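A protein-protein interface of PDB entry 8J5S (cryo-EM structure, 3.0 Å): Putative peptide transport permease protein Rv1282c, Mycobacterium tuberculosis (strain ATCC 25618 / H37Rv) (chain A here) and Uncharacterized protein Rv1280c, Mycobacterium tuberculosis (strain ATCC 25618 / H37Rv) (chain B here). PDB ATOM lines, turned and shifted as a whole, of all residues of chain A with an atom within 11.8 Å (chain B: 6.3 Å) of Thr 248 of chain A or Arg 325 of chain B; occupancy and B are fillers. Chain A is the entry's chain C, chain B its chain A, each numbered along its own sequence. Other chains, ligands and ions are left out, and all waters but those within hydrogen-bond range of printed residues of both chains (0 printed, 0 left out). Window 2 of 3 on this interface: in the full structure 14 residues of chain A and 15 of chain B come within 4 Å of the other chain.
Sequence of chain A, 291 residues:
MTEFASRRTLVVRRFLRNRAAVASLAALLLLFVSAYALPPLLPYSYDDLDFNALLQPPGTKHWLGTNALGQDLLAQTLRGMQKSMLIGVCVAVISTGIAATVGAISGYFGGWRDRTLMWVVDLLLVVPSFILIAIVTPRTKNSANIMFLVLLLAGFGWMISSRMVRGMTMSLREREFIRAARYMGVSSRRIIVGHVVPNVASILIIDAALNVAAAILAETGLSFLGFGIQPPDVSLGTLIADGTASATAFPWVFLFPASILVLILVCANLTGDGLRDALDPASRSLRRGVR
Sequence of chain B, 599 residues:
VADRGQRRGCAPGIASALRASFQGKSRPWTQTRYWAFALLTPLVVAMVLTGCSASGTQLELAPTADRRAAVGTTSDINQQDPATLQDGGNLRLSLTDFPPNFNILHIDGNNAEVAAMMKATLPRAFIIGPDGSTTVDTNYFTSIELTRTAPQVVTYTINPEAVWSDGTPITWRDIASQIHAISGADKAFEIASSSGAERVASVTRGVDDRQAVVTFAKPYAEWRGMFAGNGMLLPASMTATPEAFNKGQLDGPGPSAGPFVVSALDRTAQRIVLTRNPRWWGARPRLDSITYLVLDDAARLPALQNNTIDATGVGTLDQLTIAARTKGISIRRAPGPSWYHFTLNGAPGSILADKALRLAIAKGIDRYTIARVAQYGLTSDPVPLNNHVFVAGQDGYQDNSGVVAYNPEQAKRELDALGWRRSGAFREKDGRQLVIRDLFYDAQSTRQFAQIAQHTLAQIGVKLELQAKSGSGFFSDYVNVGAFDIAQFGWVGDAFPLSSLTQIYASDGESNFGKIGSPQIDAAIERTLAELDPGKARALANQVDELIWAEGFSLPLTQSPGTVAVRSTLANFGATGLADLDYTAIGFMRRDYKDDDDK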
ATOM      1  N   LEU A  55      19.020   8.415 -13.678  1.00  0.00           N
ATOM      2  CA  LEU A  55      17.970   7.718 -14.424  1.00  0.00           C
ATOM      3  C   LEU A  55      18.532   6.615 -15.313  1.00  0.00           C
ATOM      4  O   LEU A  55      18.148   6.467 -16.471  1.00  0.00           O
ATOM      5  CB  LEU A  55      17.141   8.707 -15.224  1.00  0.00           C
ATOM      6  CG  LEU A  55      15.984   9.230 -14.382  1.00  0.00           C
ATOM      7  CD1 LEU A  55      15.102  10.156 -15.159  1.00  0.00           C
ATOM      8  CD2 LEU A  55      15.179   8.077 -13.837  1.00  0.00           C
ATOM      9  N   ILE A 240       6.254   4.953  -4.374  1.00  0.00           N
ATOM     10  CA  ILE A 240       5.289   4.860  -5.465  1.00  0.00           C
ATOM     11  C   ILE A 240       4.798   6.241  -5.866  1.00  0.00           C
ATOM     12  O   ILE A 240       4.643   6.535  -7.056  1.00  0.00           O
ATOM     13  CB  ILE A 240       4.120   3.938  -5.088  1.00  0.00           C
ATOM     14  CG1 ILE A 240       4.626   2.700  -4.372  1.00  0.00           C
ATOM     15  CG2 ILE A 240       3.380   3.515  -6.319  1.00  0.00           C
ATOM     16  CD1 ILE A 240       3.545   1.958  -3.660  1.00  0.00           C
ATOM     17  N   ALA A 241       4.532   7.106  -4.887  1.00  0.00           N
ATOM     18  CA  ALA A 241       4.059   8.451  -5.193  1.00  0.00           C
ATOM     19  C   ALA A 241       5.086   9.228  -6.001  1.00  0.00           C
ATOM     20  O   ALA A 241       4.728   9.969  -6.919  1.00  0.00           O
ATOM     21  CB  ALA A 241       3.725   9.193  -3.905  1.00  0.00           C
ATOM     22  N   ASP A 242       6.366   9.089  -5.663  1.00  0.00           N
ATOM     23  CA  ASP A 242       7.408   9.731  -6.454  1.00  0.00           C
ATOM     24  C   ASP A 242       7.484   9.138  -7.850  1.00  0.00           C
ATOM     25  O   ASP A 242       7.691   9.863  -8.827  1.00  0.00           O
ATOM     26  CB  ASP A 242       8.760   9.599  -5.761  1.00  0.00           C
ATOM     27  CG  ASP A 242       8.759  10.175  -4.367  1.00  0.00           C
ATOM     28  OD1 ASP A 242       9.803  10.088  -3.688  1.00  0.00           O
ATOM     29  OD2 ASP A 242       7.713  10.712  -3.947  1.00  0.00           O
ATOM     30  N   GLY A 243       7.330   7.824  -7.966  1.00  0.00           N
ATOM     31  CA  GLY A 243       7.533   7.180  -9.243  1.00  0.00           C
ATOM     32  C   GLY A 243       6.370   7.222 -10.197  1.00  0.00           C
ATOM     33  O   GLY A 243       6.542   6.819 -11.348  1.00  0.00           O
ATOM     34  N   THR A 244       5.194   7.670  -9.757  1.00  0.00           N
ATOM     35  CA  THR A 244       4.056   7.752 -10.671  1.00  0.00           C
ATOM     36  C   THR A 244       4.415   8.502 -11.945  1.00  0.00           C
ATOM     37  O   THR A 244       4.160   8.025 -13.056  1.00  0.00           O
ATOM     38  CB  THR A 244       2.868   8.444 -10.009  1.00  0.00           C
ATOM     39  OG1 THR A 244       3.155   9.838  -9.865  1.00  0.00           O
ATOM     40  CG2 THR A 244       2.551   7.849  -8.672  1.00  0.00           C
ATOM     41  N   ALA A 245       5.015   9.668 -11.805  1.00  0.00           N
ATOM     42  CA  ALA A 245       5.245  10.572 -12.926  1.00  0.00           C
ATOM     43  C   ALA A 245       6.300  10.087 -13.902  1.00  0.00           C
ATOM     44  O   ALA A 245       6.628  10.836 -14.821  1.00  0.00           O
ATOM     45  CB  ALA A 245       5.627  11.953 -12.395  1.00  0.00           C
ATOM     46  N   SER A 246       6.862   8.887 -13.786  1.00  0.00           N
ATOM     47  CA  SER A 246       7.876   8.448 -14.733  1.00  0.00           C
ATOM     48  C   SER A 246       7.702   6.997 -15.155  1.00  0.00           C
ATOM     49  O   SER A 246       8.633   6.424 -15.728  1.00  0.00           O
ATOM     50  CB  SER A 246       9.269   8.647 -14.147  1.00  0.00           C
ATOM     51  OG  SER A 246       9.452   9.983 -13.722  1.00  0.00           O
ATOM     52  N   ALA A 247       6.544   6.389 -14.900  1.00  0.00           N
ATOM     53  CA  ALA A 247       6.345   4.984 -15.239  1.00  0.00           C
ATOM     54  C   ALA A 247       6.343   4.765 -16.745  1.00  0.00           C
ATOM     55  O   ALA A 247       6.803   3.726 -17.228  1.00  0.00           O
ATOM     56  CB  ALA A 247       5.038   4.486 -14.633  1.00  0.00           C
ATOM     57  N   THR A 248       5.810   5.724 -17.501  1.00  0.00           N
ATOM     58  CA  THR A 248       5.690   5.546 -18.944  1.00  0.00           C
ATOM     59  C   THR A 248       7.053   5.531 -19.623  1.00  0.00           C
ATOM     60  O   THR A 248       7.291   4.723 -20.526  1.00  0.00           O
ATOM     61  CB  THR A 248       4.821   6.653 -19.532  1.00  0.00           C
ATOM     62  OG1 THR A 248       5.615   7.828 -19.711  1.00  0.00           O
ATOM     63  CG2 THR A 248       3.671   6.975 -18.593  1.00  0.00           C
ATOM     64  N   ALA A 249       7.960   6.413 -19.202  1.00  0.00           N
ATOM     65  CA  ALA A 249       9.237   6.591 -19.880  1.00  0.00           C
ATOM     66  C   ALA A 249      10.320   5.680 -19.322  1.00  0.00           C
ATOM     67  O   ALA A 249      10.955   4.935 -20.073  1.00  0.00           O
ATOM     68  CB  ALA A 249       9.677   8.049 -19.781  1.00  0.00           C
ATOM     69  N   PHE A 250      10.549   5.739 -18.010  1.00  0.00           N
ATOM     70  CA  PHE A 250      11.502   4.879 -17.308  1.00  0.00           C
ATOM     71  C   PHE A 250      10.700   4.054 -16.317  1.00  0.00           C
ATOM     72  O   PHE A 250      10.525   4.460 -15.161  1.00  0.00           O
ATOM     73  CB  PHE A 250      12.574   5.694 -16.596  1.00  0.00           C
ATOM     74  CG  PHE A 250      12.998   6.914 -17.344  1.00  0.00           C
ATOM     75  CD1 PHE A 250      12.676   8.168 -16.893  1.00  0.00           C
ATOM     76  CD2 PHE A 250      13.734   6.807 -18.502  1.00  0.00           C
ATOM     77  CE1 PHE A 250      13.072   9.281 -17.592  1.00  0.00           C
ATOM     78  CE2 PHE A 250      14.127   7.925 -19.190  1.00  0.00           C
ATOM     79  CZ  PHE A 250      13.793   9.162 -18.729  1.00  0.00           C
ATOM     80  N   PRO A 251      10.190   2.892 -16.725  1.00  0.00           N
ATOM     81  CA  PRO A 251       9.234   2.180 -15.870  1.00  0.00           C
ATOM     82  C   PRO A 251       9.861   1.537 -14.655  1.00  0.00           C
ATOM     83  O   PRO A 251       9.130   1.181 -13.728  1.00  0.00           O
ATOM     84  CB  PRO A 251       8.646   1.129 -16.815  1.00  0.00           C
ATOM     85  CG  PRO A 251       9.721   0.882 -17.801  1.00  0.00           C
ATOM     86  CD  PRO A 251      10.468   2.166 -17.973  1.00  0.00           C
ATOM     87  N   TRP A 252      11.182   1.386 -14.612  1.00  0.00           N
ATOM     88  CA  TRP A 252      11.788   0.711 -13.478  1.00  0.00           C
ATOM     89  C   TRP A 252      11.582   1.468 -12.178  1.00  0.00           C
ATOM     90  O   TRP A 252      11.668   0.858 -11.112  1.00  0.00           O
ATOM     91  CB  TRP A 252      13.278   0.471 -13.728  1.00  0.00           C
ATOM     92  CG  TRP A 252      14.109   1.695 -13.950  1.00  0.00           C
ATOM     93  CD1 TRP A 252      14.563   2.557 -13.007  1.00  0.00           C
ATOM     94  CD2 TRP A 252      14.610   2.176 -15.201  1.00  0.00           C
ATOM     95  NE1 TRP A 252      15.302   3.551 -13.587  1.00  0.00           N
ATOM     96  CE2 TRP A 252      15.347   3.337 -14.935  1.00  0.00           C
ATOM     97  CE3 TRP A 252      14.497   1.739 -16.522  1.00  0.00           C
ATOM     98  CZ2 TRP A 252      15.960   4.070 -15.938  1.00  0.00           C
ATOM     99  CZ3 TRP A 252      15.114   2.462 -17.512  1.00  0.00           C
ATOM    100  CH2 TRP A 252      15.836   3.613 -17.218  1.00  0.00           C
ATOM    101  N   VAL A 253      11.273   2.769 -12.236  1.00  0.00           N
ATOM    102  CA  VAL A 253      11.126   3.576 -11.026  1.00  0.00           C
ATOM    103  C   VAL A 253       9.741   3.492 -10.411  1.00  0.00           C
ATOM    104  O   VAL A 253       9.556   3.942  -9.272  1.00  0.00           O
ATOM    105  CB  VAL A 253      11.441   5.063 -11.278  1.00  0.00           C
ATOM    106  CG1 VAL A 253      12.816   5.222 -11.878  1.00  0.00           C
ATOM    107  CG2 VAL A 253      10.400   5.676 -12.164  1.00  0.00           C
ATOM    108  N   PHE A 254       8.763   2.947 -11.114  1.00  0.00           N
ATOM    109  CA  PHE A 254       7.434   2.760 -10.557  1.00  0.00           C
ATOM    110  C   PHE A 254       7.004   1.311 -10.504  1.00  0.00           C
ATOM    111  O   PHE A 254       6.299   0.925  -9.575  1.00  0.00           O
ATOM    112  CB  PHE A 254       6.395   3.550 -11.363  1.00  0.00           C
ATOM    113  CG  PHE A 254       4.979   3.123 -11.116  1.00  0.00           C
ATOM    114  CD1 PHE A 254       4.293   3.560 -10.007  1.00  0.00           C
ATOM    115  CD2 PHE A 254       4.330   2.291 -11.999  1.00  0.00           C
ATOM    116  CE1 PHE A 254       2.989   3.170  -9.784  1.00  0.00           C
ATOM    117  CE2 PHE A 254       3.029   1.896 -11.780  1.00  0.00           C
ATOM    118  CZ  PHE A 254       2.359   2.337 -10.671  1.00  0.00           C
ATOM    119  N   LEU A 255       7.406   0.498 -11.477  1.00  0.00           N
ATOM    120  CA  LEU A 255       6.980  -0.891 -11.496  1.00  0.00           C
ATOM    121  C   LEU A 255       7.595  -1.678 -10.362  1.00  0.00           C
ATOM    122  O   LEU A 255       7.001  -2.653  -9.901  1.00  0.00           O
ATOM    123  CB  LEU A 255       7.340  -1.536 -12.830  1.00  0.00           C
ATOM    124  CG  LEU A 255       6.573  -1.043 -14.052  1.00  0.00           C
ATOM    125  CD1 LEU A 255       6.600  -2.094 -15.132  1.00  0.00           C
ATOM    126  CD2 LEU A 255       5.148  -0.696 -13.684  1.00  0.00           C
ATOM    127  N   PHE A 256       8.766  -1.294  -9.906  1.00  0.00           N
ATOM    128  CA  PHE A 256       9.402  -2.131  -8.905  1.00  0.00           C
ATOM    129  C   PHE A 256       8.814  -1.952  -7.503  1.00  0.00           C
ATOM    130  O   PHE A 256       8.381  -2.945  -6.905  1.00  0.00           O
ATOM    131  CB  PHE A 256      10.902  -1.900  -8.882  1.00  0.00           C
ATOM    132  CG  PHE A 256      11.624  -2.937  -8.125  1.00  0.00           C
ATOM    133  CD1 PHE A 256      11.048  -4.169  -7.900  1.00  0.00           C
ATOM    134  CD2 PHE A 256      12.825  -2.674  -7.554  1.00  0.00           C
ATOM    135  CE1 PHE A 256      11.693  -5.132  -7.170  1.00  0.00           C
ATOM    136  CE2 PHE A 256      13.440  -3.629  -6.804  1.00  0.00           C
ATOM    137  CZ  PHE A 256      12.901  -4.855  -6.631  1.00  0.00           C
ATOM    138  N   ALA A 258       5.986  -0.748  -6.606  1.00  0.00           N
ATOM    139  CA  ALA A 258       4.589  -1.150  -6.650  1.00  0.00           C
ATOM    140  C   ALA A 258       4.455  -2.660  -6.683  1.00  0.00           C
ATOM    141  O   ALA A 258       3.598  -3.227  -5.997  1.00  0.00           O
ATOM    142  CB  ALA A 258       3.900  -0.523  -7.857  1.00  0.00           C
ATOM    143  N   GLN B 305      -1.248  14.554 -23.532  1.00  0.00           N
ATOM    144  CA  GLN B 305      -1.240  13.275 -24.230  1.00  0.00           C
ATOM    145  C   GLN B 305      -2.633  12.888 -24.694  1.00  0.00           C
ATOM    146  O   GLN B 305      -2.809  12.414 -25.821  1.00  0.00           O
ATOM    147  CB  GLN B 305      -0.667  12.185 -23.331  1.00  0.00           C
ATOM    148  CG  GLN B 305       0.722  12.460 -22.819  1.00  0.00           C
ATOM    149  CD  GLN B 305       1.547  11.205 -22.666  1.00  0.00           C
ATOM    150  OE1 GLN B 305       2.086  10.685 -23.633  1.00  0.00           O
ATOM    151  NE2 GLN B 305       1.645  10.709 -21.445  1.00  0.00           N
ATOM    152  N   ASP B 318      11.294  13.619 -18.002  1.00  0.00           N
ATOM    153  CA  ASP B 318      10.085  12.886 -18.370  1.00  0.00           C
ATOM    154  C   ASP B 318       9.113  13.757 -19.138  1.00  0.00           C
ATOM    155  O   ASP B 318       8.492  13.305 -20.103  1.00  0.00           O
ATOM    156  CB  ASP B 318       9.385  12.348 -17.132  1.00  0.00           C
ATOM    157  CG  ASP B 318      10.323  11.668 -16.195  1.00  0.00           C
ATOM    158  OD1 ASP B 318      10.472  12.130 -15.048  1.00  0.00           O
ATOM    159  OD2 ASP B 318      10.894  10.647 -16.599  1.00  0.00           O
ATOM    160  N   LEU B 320       9.748  15.914 -21.115  1.00  0.00           N
ATOM    161  CA  LEU B 320      10.293  16.036 -22.457  1.00  0.00           C
ATOM    162  C   LEU B 320      10.207  14.737 -23.241  1.00  0.00           C
ATOM    163  O   LEU B 320       9.960  14.768 -24.449  1.00  0.00           O
ATOM    164  CB  LEU B 320      11.741  16.504 -22.388  1.00  0.00           C
ATOM    165  CG  LEU B 320      12.627  16.293 -23.606  1.00  0.00           C
ATOM    166  CD1 LEU B 320      12.249  17.250 -24.694  1.00  0.00           C
ATOM    167  CD2 LEU B 320      14.071  16.486 -23.221  1.00  0.00           C
ATOM    168  N   THR B 321      10.417  13.589 -22.596  1.00  0.00           N
ATOM    169  CA  THR B 321      10.248  12.326 -23.304  1.00  0.00           C
ATOM    170  C   THR B 321       8.796  12.121 -23.692  1.00  0.00           C
ATOM    171  O   THR B 321       8.492  11.824 -24.852  1.00  0.00           O
ATOM    172  CB  THR B 321      10.731  11.148 -22.467  1.00  0.00           C
ATOM    173  OG1 THR B 321       9.711  10.787 -21.536  1.00  0.00           O
ATOM    174  CG2 THR B 321      12.004  11.480 -21.738  1.00  0.00           C
ATOM    175  N   ILE B 322       7.873  12.279 -22.746  1.00  0.00           N
ATOM    176  CA  ILE B 322       6.483  12.140 -23.143  1.00  0.00           C
ATOM    177  C   ILE B 322       5.975  13.504 -23.589  1.00  0.00           C
ATOM    178  O   ILE B 322       4.974  14.028 -23.090  1.00  0.00           O
ATOM    179  CB  ILE B 322       5.659  11.545 -21.984  1.00  0.00           C
ATOM    180  CG1 ILE B 322       5.537  12.498 -20.802  1.00  0.00           C
ATOM    181  CG2 ILE B 322       6.363  10.367 -21.423  1.00  0.00           C
ATOM    182  CD1 ILE B 322       4.319  12.261 -19.969  1.00  0.00           C
ATOM    183  N   ALA B 323       6.610  14.031 -24.611  1.00  0.00           N
ATOM    184  CA  ALA B 323       6.066  15.052 -25.489  1.00  0.00           C
ATOM    185  C   ALA B 323       6.514  14.876 -26.924  1.00  0.00           C
ATOM    186  O   ALA B 323       5.800  15.304 -27.833  1.00  0.00           O
ATOM    187  CB  ALA B 323       6.461  16.447 -25.002  1.00  0.00           C
ATOM    188  N   ALA B 324       7.665  14.248 -27.156  1.00  0.00           N
ATOM    189  CA  ALA B 324       8.130  13.883 -28.478  1.00  0.00           C
ATOM    190  C   ALA B 324       8.036  12.393 -28.737  1.00  0.00           C
ATOM    191  O   ALA B 324       8.122  11.976 -29.895  1.00  0.00           O
ATOM    192  CB  ALA B 324       9.583  14.334 -28.679  1.00  0.00           C
ATOM    193  N   ARG B 325       7.864  11.585 -27.694  1.00  0.00           N
ATOM    194  CA  ARG B 325       7.540  10.183 -27.890  1.00  0.00           C
ATOM    195  C   ARG B 325       6.110   9.983 -28.359  1.00  0.00           C
ATOM    196  O   ARG B 325       5.767   8.879 -28.796  1.00  0.00           O
ATOM    197  CB  ARG B 325       7.763   9.416 -26.598  1.00  0.00           C
ATOM    198  CG  ARG B 325       9.171   8.926 -26.384  1.00  0.00           C
ATOM    199  CD  ARG B 325       9.185   7.637 -25.591  1.00  0.00           C
ATOM    200  NE  ARG B 325       8.571   7.759 -24.272  1.00  0.00           N
ATOM    201  CZ  ARG B 325       7.287   7.536 -24.012  1.00  0.00           C
ATOM    202  NH1 ARG B 325       6.828   7.665 -22.780  1.00  0.00           N
ATOM    203  NH2 ARG B 325       6.460   7.177 -24.979  1.00  0.00           N
ATOM    204  N   THR B 326       5.278  11.009 -28.264  1.00  0.00           N
ATOM    205  CA  THR B 326       3.924  10.991 -28.782  1.00  0.00           C
ATOM    206  C   THR B 326       3.872  11.698 -30.126  1.00  0.00           C
ATOM    207  O   THR B 326       4.819  12.360 -30.550  1.00  0.00           O
ATOM    208  CB  THR B 326       2.961  11.650 -27.803  1.00  0.00           C
ATOM    209  OG1 THR B 326       3.028  13.062 -27.967  1.00  0.00           O
ATOM    210  CG2 THR B 326       3.350  11.308 -26.398  1.00  0.00           C
ATOM    211  N   LYS B 327       2.737  11.557 -30.796  1.00  0.00           N
ATOM    212  CA  LYS B 327       2.557  12.053 -32.147  1.00  0.00           C
ATOM    213  C   LYS B 327       1.588  13.227 -32.150  1.00  0.00           C
ATOM    214  O   LYS B 327       0.669  13.302 -31.332  1.00  0.00           O
ATOM    215  CB  LYS B 327       2.051  10.943 -33.072  1.00  0.00           C
ATOM    216  CG  LYS B 327       2.793   9.619 -32.921  1.00  0.00           C
ATOM    217  CD  LYS B 327       2.106   8.703 -31.918  1.00  0.00           C
ATOM    218  CE  LYS B 327       2.711   7.311 -31.925  1.00  0.00           C
ATOM    219  NZ  LYS B 327       2.164   6.457 -30.834  1.00  0.00           N
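The guanidinium group (NH1) of Arg 325 of chain B is in hydrogen-bond range of the side-chain hydroxyl (OG1) of Thr 248 of chain A (3.3 Å). OD1 of Asp 318 of chain B lies within hydrogen-bond range of OG of Ser 246 of chain A (2.7 Å).
The side-chain hydroxyl (OG1) of Thr 321 of chain B sits at hydrogen-bond distance from the backbone carbonyl oxygen (O) of Asp 318 of chain B, at 3.1 Å.
Among the printed residues, merely in contact across the chains: Phe 250 of chain A with Asp 318 of chain B, Thr 248 of chain A with Ile 322 of chain B, Ala 249 of chain A with Thr 321 of chain B, Ala 245 of chain A with Asp 318 of chain B and Ala 249 of chain A with Arg 325 of chain B.
Ile 240 of chain A touches none of the printed residues of chain B. Of the printed residues of chain B, Ala 245 of chain A touches Asp 318. Printed residues of chain B within 4 Å of Ser 246 of chain A: Asp 318. Thr 248 of chain A touches two residues of chain B. Printed residues of chain B within 4 Å of Ala 249 of chain A: Thr 321 and Arg 325. Of the printed residues of chain B, Phe 250 of chain A touches Asp 318 (2.8 Å). Gln 305 of chain B touches none of the printed residues of chain A. Printed residues of chain A within 4 Å of Asp 318 of chain B: Ala 245 (3.9 Å), Ser 246 (2.7 Å) and Phe 250 (2.8 Å). Of chain A, only Ala 249 (3.3 Å) comes within 4 Å of Thr 321 of chain B. Of the printed residues of chain A, Ile 322 of chain B touches Thr 248 (3.2 Å). No residue of chain A comes within 4 Å of Ala 324 of chain B. Of chain A, only Thr 248 and Ala 249 come within 4 Å of Arg 325 of chain B. No residue of chain A comes within 4 Å of Thr 326 of chain B. No residue of chain A comes within 4 Å of Lys 327 of chain B. The nearest printed residue of chain B that does not touch Ala 249 of chain A is Asp 318 of chain B (4.3 Å).
Of the 10 printed residues of chain B, 4 touch a printed residue of chain A. Hydrophobic or aromatic side chains of chain B that line the printed part of chain A: Ile 322. Among the printed residues, no Asp or Glu carboxylate lies within 4 Å of a Lys or Arg side-chain nitrogen of the other chain.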
